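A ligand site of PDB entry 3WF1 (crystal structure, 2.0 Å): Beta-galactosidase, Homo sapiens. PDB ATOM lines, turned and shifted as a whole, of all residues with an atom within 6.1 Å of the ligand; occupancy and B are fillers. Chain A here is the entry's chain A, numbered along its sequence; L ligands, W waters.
The side-chain carboxylate of Glu 130 lies within hydrogen-bond range of an oxygen (O3) of the ligand. The side-chain carboxylate of Glu 269 sits at hydrogen-bond distance from an oxygen (O2) of the ligand. An oxygen (O1) of the ligand sits at hydrogen-bond distance from the side-chain carboxylate (OE1) of Glu 189, 2.7 Å away. OH of Tyr 84 lies within hydrogen-bond range of O4 of the ligand. An oxygen (O4) of the ligand sits at hydrogen-bond distance from the backbone NH (N) of Ala 129, 2.8 Å away. The side-chain amide nitrogen (ND2) of Asn 188 lies within hydrogen-bond range of an oxygen (O2) of the ligand, 2.9 Å away. OH of Tyr 334 sits close to S1 of the ligand (3.2 Å). O of Ile 127 lies within hydrogen-bond range of O4 of the ligand (3.1 Å). SG of Cys 128 is in hydrogen-bond range of O3 of the ligand (3.2 Å).
The side-chain carboxylate of Glu 269 sits at hydrogen-bond distance from the side-chain hydroxyl of Tyr 84. The side-chain hydroxyl of Tyr 271 lies within hydrogen-bond range of the side-chain carboxylate of Glu 269 (2.6 Å). OE2 of Glu 269 is in salt-bridge range of NH1 of Arg 122, at 3.1 Å. The side-chain carboxylate (OE2) of Glu 189 lies close to the side-chain carboxylate (OD2) of Asp 242. The backbone NH (N) of Glu 189 lies within hydrogen-bond range of the backbone carbonyl oxygen (O) of Thr 221. O of Tyr 334 lies within hydrogen-bond range of N of Trp 274 (3.2 Å). The side-chain amide oxygen (OD1) of Asn 485 is in hydrogen-bond range of the side-chain sulfur (SG) of Cys 128 (3.3 Å). The side-chain hydroxyl (OH) of Tyr 271 sits close to the side-chain carboxylate (OD2) of Asp 242 (3.4 Å).
Residues that only touch the ligand: Tyr 271, Trp 274, Leu 275, Tyr 307 and Tyr 486. Hydrophobic or aromatic side chains that line the ligand: Tyr 84, Ala 129, Tyr 271, Trp 274, Leu 275 and Tyr 307. Within 4 Å of the ligand: Tyr 84, Ile 127, Cys 128, Ala 129, Glu 130, Asn 188, Glu 189, Glu 269, Tyr 271, Trp 274, Leu 275, Tyr 307, Tyr 334 and Tyr 486. The nearest printed residue that does not touch the ligand is Asp 242 (4.3 Å).
Water W2 lies within hydrogen-bond range of O1 of the ligand (2.9 Å) and SG of Cys 128 (3.4 Å). Water W1 lies within hydrogen-bond range of OE1 of Glu 189 (2.8 Å) and OH of Tyr 486 (2.9 Å).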
ATOM      1  N   TYR A  84      17.912  -6.396 -20.920  1.00  0.00           N
ATOM      2  CA  TYR A  84      18.355  -6.233 -19.549  1.00  0.00           C
ATOM      3  C   TYR A  84      19.044  -4.842 -19.400  1.00  0.00           C
ATOM      4  O   TYR A  84      19.637  -4.297 -20.326  1.00  0.00           O
ATOM      5  CB  TYR A  84      19.401  -7.297 -19.233  1.00  0.00           C
ATOM      6  CG  TYR A  84      18.951  -8.697 -18.906  1.00  0.00           C
ATOM      7  CD1 TYR A  84      18.082  -8.942 -17.819  1.00  0.00           C
ATOM      8  CD2 TYR A  84      19.471  -9.782 -19.575  1.00  0.00           C
ATOM      9  CE1 TYR A  84      17.732 -10.228 -17.461  1.00  0.00           C
ATOM     10  CE2 TYR A  84      19.124 -11.080 -19.243  1.00  0.00           C
ATOM     11  CZ  TYR A  84      18.243 -11.301 -18.169  1.00  0.00           C
ATOM     12  OH  TYR A  84      17.934 -12.612 -17.826  1.00  0.00           O
ATOM     13  N   ARG A 122      13.873  -5.606 -18.290  1.00  0.00           N
ATOM     14  CA  ARG A 122      14.424  -6.329 -17.179  1.00  0.00           C
ATOM     15  C   ARG A 122      15.614  -5.595 -16.516  1.00  0.00           C
ATOM     16  O   ARG A 122      16.766  -5.842 -16.866  1.00  0.00           O
ATOM     17  CB  ARG A 122      14.751  -7.741 -17.630  1.00  0.00           C
ATOM     18  CG  ARG A 122      13.613  -8.284 -18.498  1.00  0.00           C
ATOM     19  CD  ARG A 122      13.544  -9.766 -18.511  1.00  0.00           C
ATOM     20  NE  ARG A 122      14.625 -10.406 -19.278  1.00  0.00           N
ATOM     21  CZ  ARG A 122      14.971 -11.673 -19.122  1.00  0.00           C
ATOM     22  NH1 ARG A 122      14.354 -12.424 -18.193  1.00  0.00           N
ATOM     23  NH2 ARG A 122      15.931 -12.189 -19.841  1.00  0.00           N
ATOM     24  N   ILE A 127      20.922  -9.317 -13.152  1.00  0.00           N
ATOM     25  CA  ILE A 127      20.371  -9.840 -14.406  1.00  0.00           C
ATOM     26  C   ILE A 127      20.959 -11.185 -14.905  1.00  0.00           C
ATOM     27  O   ILE A 127      20.437 -11.722 -15.900  1.00  0.00           O
ATOM     28  CB  ILE A 127      20.550  -8.828 -15.556  1.00  0.00           C
ATOM     29  CG1 ILE A 127      22.047  -8.513 -15.754  1.00  0.00           C
ATOM     30  CG2 ILE A 127      19.740  -7.566 -15.272  1.00  0.00           C
ATOM     31  CD1 ILE A 127      22.329  -7.796 -17.056  1.00  0.00           C
ATOM     32  N   CYS A 128      22.032 -11.704 -14.262  1.00  0.00           N
ATOM     33  CA  CYS A 128      22.729 -12.965 -14.677  1.00  0.00           C
ATOM     34  C   CYS A 128      23.349 -12.780 -16.076  1.00  0.00           C
ATOM     35  O   CYS A 128      24.410 -12.134 -16.191  1.00  0.00           O
ATOM     36  CB  CYS A 128      21.772 -14.184 -14.613  1.00  0.00           C
ATOM     37  SG  CYS A 128      22.441 -15.848 -14.928  1.00  0.00           S
ATOM     38  N   ALA A 129      22.737 -13.366 -17.106  1.00  0.00           N
ATOM     39  CA  ALA A 129      22.892 -12.884 -18.481  1.00  0.00           C
ATOM     40  C   ALA A 129      24.249 -13.122 -19.108  1.00  0.00           C
ATOM     41  O   ALA A 129      24.588 -12.437 -20.094  1.00  0.00           O
ATOM     42  CB  ALA A 129      22.587 -11.392 -18.523  1.00  0.00           C
ATOM     43  N   GLU A 130      25.022 -14.067 -18.558  1.00  0.00           N
ATOM     44  CA  GLU A 130      26.435 -14.303 -18.969  1.00  0.00           C
ATOM     45  C   GLU A 130      27.211 -12.959 -19.047  1.00  0.00           C
ATOM     46  O   GLU A 130      28.096 -12.708 -19.917  1.00  0.00           O
ATOM     47  CB  GLU A 130      26.522 -15.036 -20.314  1.00  0.00           C
ATOM     48  CG  GLU A 130      25.998 -16.496 -20.349  1.00  0.00           C
ATOM     49  CD  GLU A 130      24.514 -16.629 -20.139  1.00  0.00           C
ATOM     50  OE1 GLU A 130      23.677 -16.226 -20.999  1.00  0.00           O
ATOM     51  OE2 GLU A 130      24.161 -17.148 -19.081  1.00  0.00           O
ATOM     52  N   ASN A 188      15.981 -11.448 -11.145  1.00  0.00           N
ATOM     53  CA  ASN A 188      16.168 -12.418 -12.185  1.00  0.00           C
ATOM     54  C   ASN A 188      16.400 -13.822 -11.630  1.00  0.00           C
ATOM     55  O   ASN A 188      17.428 -14.081 -10.961  1.00  0.00           O
ATOM     56  CB  ASN A 188      17.328 -12.033 -13.130  1.00  0.00           C
ATOM     57  CG  ASN A 188      17.311 -12.896 -14.365  1.00  0.00           C
ATOM     58  OD1 ASN A 188      16.568 -12.604 -15.344  1.00  0.00           O
ATOM     59  ND2 ASN A 188      17.998 -14.037 -14.290  1.00  0.00           N
ATOM     60  N   GLU A 189      15.420 -14.691 -11.820  1.00  0.00           N
ATOM     61  CA  GLU A 189      15.443 -16.062 -11.264  1.00  0.00           C
ATOM     62  C   GLU A 189      15.919 -16.083  -9.829  1.00  0.00           C
ATOM     63  O   GLU A 189      16.789 -16.867  -9.465  1.00  0.00           O
ATOM     64  CB  GLU A 189      16.319 -16.962 -12.156  1.00  0.00           C
ATOM     65  CG  GLU A 189      15.845 -17.032 -13.604  1.00  0.00           C
ATOM     66  CD  GLU A 189      16.679 -17.958 -14.481  1.00  0.00           C
ATOM     67  OE1 GLU A 189      17.904 -18.080 -14.240  1.00  0.00           O
ATOM     68  OE2 GLU A 189      16.123 -18.584 -15.424  1.00  0.00           O
ATOM     69  N   THR A 221      10.604 -14.072 -13.112  1.00  0.00           N
ATOM     70  CA  THR A 221      10.905 -15.172 -13.963  1.00  0.00           C
ATOM     71  C   THR A 221      11.749 -16.191 -13.239  1.00  0.00           C
ATOM     72  O   THR A 221      12.714 -15.824 -12.577  1.00  0.00           O
ATOM     73  CB  THR A 221      11.652 -14.725 -15.232  1.00  0.00           C
ATOM     74  OG1 THR A 221      10.846 -13.757 -15.875  1.00  0.00           O
ATOM     75  CG2 THR A 221      11.864 -15.959 -16.189  1.00  0.00           C
ATOM     76  N   PHE A 228      12.195 -24.126  -8.002  1.00  0.00           N
ATOM     77  CA  PHE A 228      12.648 -22.764  -8.311  1.00  0.00           C
ATOM     78  C   PHE A 228      11.607 -21.705  -7.962  1.00  0.00           C
ATOM     79  O   PHE A 228      11.955 -20.616  -7.476  1.00  0.00           O
ATOM     80  CB  PHE A 228      13.009 -22.640  -9.775  1.00  0.00           C
ATOM     81  CG  PHE A 228      14.171 -23.533 -10.201  1.00  0.00           C
ATOM     82  CD1 PHE A 228      15.422 -23.374  -9.647  1.00  0.00           C
ATOM     83  CD2 PHE A 228      13.997 -24.497 -11.168  1.00  0.00           C
ATOM     84  CE1 PHE A 228      16.473 -24.181 -10.015  1.00  0.00           C
ATOM     85  CE2 PHE A 228      15.045 -25.301 -11.552  1.00  0.00           C
ATOM     86  CZ  PHE A 228      16.285 -25.145 -10.968  1.00  0.00           C
ATOM     87  N   ASP A 242      10.601 -19.796 -17.456  1.00  0.00           N
ATOM     88  CA  ASP A 242      11.406 -19.937 -18.664  1.00  0.00           C
ATOM     89  C   ASP A 242      11.733 -21.412 -18.901  1.00  0.00           C
ATOM     90  O   ASP A 242      11.754 -22.199 -17.961  1.00  0.00           O
ATOM     91  CB  ASP A 242      12.694 -19.031 -18.675  1.00  0.00           C
ATOM     92  CG  ASP A 242      13.602 -19.193 -17.455  1.00  0.00           C
ATOM     93  OD1 ASP A 242      13.735 -20.294 -16.931  1.00  0.00           O
ATOM     94  OD2 ASP A 242      14.196 -18.173 -17.004  1.00  0.00           O
ATOM     95  N   GLU A 269      11.911 -16.645 -21.330  1.00  0.00           N
ATOM     96  CA  GLU A 269      13.183 -16.977 -21.987  1.00  0.00           C
ATOM     97  C   GLU A 269      13.081 -18.349 -22.622  1.00  0.00           C
ATOM     98  O   GLU A 269      13.440 -19.350 -22.023  1.00  0.00           O
ATOM     99  CB  GLU A 269      14.370 -16.992 -21.012  1.00  0.00           C
ATOM    100  CG  GLU A 269      14.513 -15.807 -20.062  1.00  0.00           C
ATOM    101  CD  GLU A 269      15.800 -15.870 -19.257  1.00  0.00           C
ATOM    102  OE1 GLU A 269      16.516 -16.899 -19.423  1.00  0.00           O
ATOM    103  OE2 GLU A 269      16.107 -14.924 -18.454  1.00  0.00           O
ATOM    104  N   TYR A 271      14.736 -20.556 -25.020  1.00  0.00           N
ATOM    105  CA  TYR A 271      16.125 -20.587 -25.558  1.00  0.00           C
ATOM    106  C   TYR A 271      16.219 -21.001 -27.052  1.00  0.00           C
ATOM    107  O   TYR A 271      15.855 -22.117 -27.411  1.00  0.00           O
ATOM    108  CB  TYR A 271      17.052 -21.429 -24.662  1.00  0.00           C
ATOM    109  CG  TYR A 271      16.891 -20.968 -23.251  1.00  0.00           C
ATOM    110  CD1 TYR A 271      17.320 -19.697 -22.869  1.00  0.00           C
ATOM    111  CD2 TYR A 271      16.222 -21.742 -22.318  1.00  0.00           C
ATOM    112  CE1 TYR A 271      17.097 -19.211 -21.592  1.00  0.00           C
ATOM    113  CE2 TYR A 271      16.042 -21.274 -20.997  1.00  0.00           C
ATOM    114  CZ  TYR A 271      16.443 -20.002 -20.658  1.00  0.00           C
ATOM    115  OH  TYR A 271      16.247 -19.485 -19.369  1.00  0.00           O
ATOM    116  N   TRP A 274      22.258 -21.387 -27.214  1.00  0.00           N
ATOM    117  CA  TRP A 274      22.865 -21.513 -25.873  1.00  0.00           C
ATOM    118  C   TRP A 274      24.284 -20.919 -25.806  1.00  0.00           C
ATOM    119  O   TRP A 274      24.999 -20.822 -26.820  1.00  0.00           O
ATOM    120  CB  TRP A 274      22.920 -23.000 -25.457  1.00  0.00           C
ATOM    121  CG  TRP A 274      23.020 -23.252 -23.992  1.00  0.00           C
ATOM    122  CD1 TRP A 274      24.105 -23.726 -23.321  1.00  0.00           C
ATOM    123  CD2 TRP A 274      22.004 -23.049 -23.014  1.00  0.00           C
ATOM    124  NE1 TRP A 274      23.835 -23.837 -21.993  1.00  0.00           N
ATOM    125  CE2 TRP A 274      22.545 -23.428 -21.770  1.00  0.00           C
ATOM    126  CE3 TRP A 274      20.682 -22.587 -23.068  1.00  0.00           C
ATOM    127  CZ2 TRP A 274      21.806 -23.366 -20.565  1.00  0.00           C
ATOM    128  CZ3 TRP A 274      19.946 -22.536 -21.889  1.00  0.00           C
ATOM    129  CH2 TRP A 274      20.511 -22.918 -20.648  1.00  0.00           C
ATOM    130  N   LEU A 275      24.660 -20.566 -24.574  1.00  0.00           N
ATOM    131  CA  LEU A 275      25.917 -19.895 -24.272  1.00  0.00           C
ATOM    132  C   LEU A 275      27.114 -20.784 -24.532  1.00  0.00           C
ATOM    133  O   LEU A 275      27.008 -22.019 -24.598  1.00  0.00           O
ATOM    134  CB  LEU A 275      25.899 -19.431 -22.800  1.00  0.00           C
ATOM    135  CG  LEU A 275      25.786 -20.475 -21.682  1.00  0.00           C
ATOM    136  CD1 LEU A 275      27.114 -20.572 -20.935  1.00  0.00           C
ATOM    137  CD2 LEU A 275      24.689 -20.167 -20.659  1.00  0.00           C
ATOM    138  N   TYR A 307      14.975 -15.962 -26.298  1.00  0.00           N
ATOM    139  CA  TYR A 307      16.291 -15.639 -25.678  1.00  0.00           C
ATOM    140  C   TYR A 307      17.405 -16.490 -26.338  1.00  0.00           C
ATOM    141  O   TYR A 307      17.396 -17.700 -26.233  1.00  0.00           O
ATOM    142  CB  TYR A 307      16.252 -15.918 -24.155  1.00  0.00           C
ATOM    143  CG  TYR A 307      17.417 -15.351 -23.388  1.00  0.00           C
ATOM    144  CD1 TYR A 307      18.680 -15.950 -23.451  1.00  0.00           C
ATOM    145  CD2 TYR A 307      17.305 -14.148 -22.686  1.00  0.00           C
ATOM    146  CE1 TYR A 307      19.768 -15.393 -22.822  1.00  0.00           C
ATOM    147  CE2 TYR A 307      18.400 -13.571 -22.049  1.00  0.00           C
ATOM    148  CZ  TYR A 307      19.626 -14.223 -22.108  1.00  0.00           C
ATOM    149  OH  TYR A 307      20.746 -13.694 -21.517  1.00  0.00           O
ATOM    150  N   TYR A 332      28.851 -13.359 -28.101  1.00  0.00           N
ATOM    151  CA  TYR A 332      27.580 -13.817 -27.557  1.00  0.00           C
ATOM    152  C   TYR A 332      26.644 -14.170 -28.705  1.00  0.00           C
ATOM    153  O   TYR A 332      25.397 -13.987 -28.609  1.00  0.00           O
ATOM    154  CB  TYR A 332      26.938 -12.750 -26.683  1.00  0.00           C
ATOM    155  CG  TYR A 332      25.942 -13.275 -25.641  1.00  0.00           C
ATOM    156  CD1 TYR A 332      26.295 -14.251 -24.719  1.00  0.00           C
ATOM    157  CD2 TYR A 332      24.656 -12.782 -25.572  1.00  0.00           C
ATOM    158  CE1 TYR A 332      25.401 -14.723 -23.744  1.00  0.00           C
ATOM    159  CE2 TYR A 332      23.753 -13.216 -24.608  1.00  0.00           C
ATOM    160  CZ  TYR A 332      24.108 -14.184 -23.697  1.00  0.00           C
ATOM    161  OH  TYR A 332      23.193 -14.609 -22.730  1.00  0.00           O
ATOM    162  N   TYR A 334      25.440 -16.913 -29.653  1.00  0.00           N
ATOM    163  CA  TYR A 334      24.390 -17.717 -28.968  1.00  0.00           C
ATOM    164  C   TYR A 334      23.646 -18.624 -29.946  1.00  0.00           C
ATOM    165  O   TYR A 334      22.682 -19.228 -29.575  1.00  0.00           O
ATOM    166  CB  TYR A 334      23.385 -16.776 -28.281  1.00  0.00           C
ATOM    167  CG  TYR A 334      22.755 -17.310 -27.006  1.00  0.00           C
ATOM    168  CD1 TYR A 334      23.384 -17.128 -25.801  1.00  0.00           C
ATOM    169  CD2 TYR A 334      21.543 -18.027 -27.033  1.00  0.00           C
ATOM    170  CE1 TYR A 334      22.854 -17.626 -24.625  1.00  0.00           C
ATOM    171  CE2 TYR A 334      20.981 -18.543 -25.860  1.00  0.00           C
ATOM    172  CZ  TYR A 334      21.665 -18.346 -24.656  1.00  0.00           C
ATOM    173  OH  TYR A 334      21.137 -18.830 -23.478  1.00  0.00           O
ATOM    174  N   ASN A 485      28.647 -14.978 -12.782  1.00  0.00           N
ATOM    175  CA  ASN A 485      27.345 -14.294 -12.902  1.00  0.00           C
ATOM    176  C   ASN A 485      26.151 -15.153 -12.450  1.00  0.00           C
ATOM    177  O   ASN A 485      25.003 -14.714 -12.598  1.00  0.00           O
ATOM    178  CB  ASN A 485      27.068 -13.870 -14.362  1.00  0.00           C
ATOM    179  CG  ASN A 485      26.858 -15.062 -15.309  1.00  0.00           C
ATOM    180  OD1 ASN A 485      25.720 -15.565 -15.516  1.00  0.00           O
ATOM    181  ND2 ASN A 485      27.947 -15.536 -15.853  1.00  0.00           N
ATOM    182  N   TYR A 486      26.427 -16.377 -11.994  1.00  0.00           N
ATOM    183  CA  TYR A 486      25.358 -17.292 -11.557  1.00  0.00           C
ATOM    184  C   TYR A 486      25.850 -18.218 -10.478  1.00  0.00           C
ATOM    185  O   TYR A 486      26.955 -18.728 -10.576  1.00  0.00           O
ATOM    186  CB  TYR A 486      24.824 -18.079 -12.722  1.00  0.00           C
ATOM    187  CG  TYR A 486      23.674 -19.034 -12.455  1.00  0.00           C
ATOM    188  CD1 TYR A 486      22.385 -18.548 -12.275  1.00  0.00           C
ATOM    189  CD2 TYR A 486      23.872 -20.405 -12.481  1.00  0.00           C
ATOM    190  CE1 TYR A 486      21.320 -19.408 -12.049  1.00  0.00           C
ATOM    191  CE2 TYR A 486      22.812 -21.299 -12.278  1.00  0.00           C
ATOM    192  CZ  TYR A 486      21.539 -20.789 -12.067  1.00  0.00           C
ATOM    193  OH  TYR A 486      20.483 -21.635 -11.846  1.00  0.00           O
HETATM  194  C1  LIG L   1      18.829 -17.937 -17.620  1.00  0.00           C
HETATM  195  O1  LIG L   1      19.401 -18.499 -16.430  1.00  0.00           O
HETATM  196  C2  LIG L   1      18.942 -16.428 -17.333  1.00  0.00           C
HETATM  197  O2  LIG L   1      17.827 -15.844 -16.615  1.00  0.00           O
HETATM  198  N1  LIG L   1      19.703 -18.413 -18.686  1.00  0.00           N
HETATM  199  C3  LIG L   1      19.842 -19.698 -19.044  1.00  0.00           C
HETATM  200  N2  LIG L   1      19.402 -20.797 -18.492  1.00  0.00           N
HETATM  201  C4  LIG L   1      18.629 -21.239 -17.307  1.00  0.00           C
HETATM  202  C5  LIG L   1      19.636 -21.643 -16.201  1.00  0.00           C
HETATM  203  C6  LIG L   1      20.073 -23.114 -16.224  1.00  0.00           C
HETATM  204  C7  LIG L   1      20.412 -23.658 -14.843  1.00  0.00           C
HETATM  205  S1  LIG L   1      20.699 -19.810 -20.486  1.00  0.00           S
HETATM  206  C8  LIG L   1      21.402 -18.197 -20.467  1.00  0.00           C
HETATM  207  C9  LIG L   1      20.347 -17.442 -19.617  1.00  0.00           C
HETATM  208  C10 LIG L   1      20.927 -16.218 -18.892  1.00  0.00           C
HETATM  209  O3  LIG L   1      21.975 -16.580 -17.987  1.00  0.00           O
HETATM  210  C11 LIG L   1      19.762 -15.491 -18.283  1.00  0.00           C
HETATM  211  O4  LIG L   1      20.153 -14.250 -17.681  1.00  0.00           O
HETATM  212  O   HOH W   1      18.066 -20.736 -13.241  1.00  0.00           O
HETATM  213  O   HOH W   2      22.212 -19.052 -16.065  1.00  0.00           O
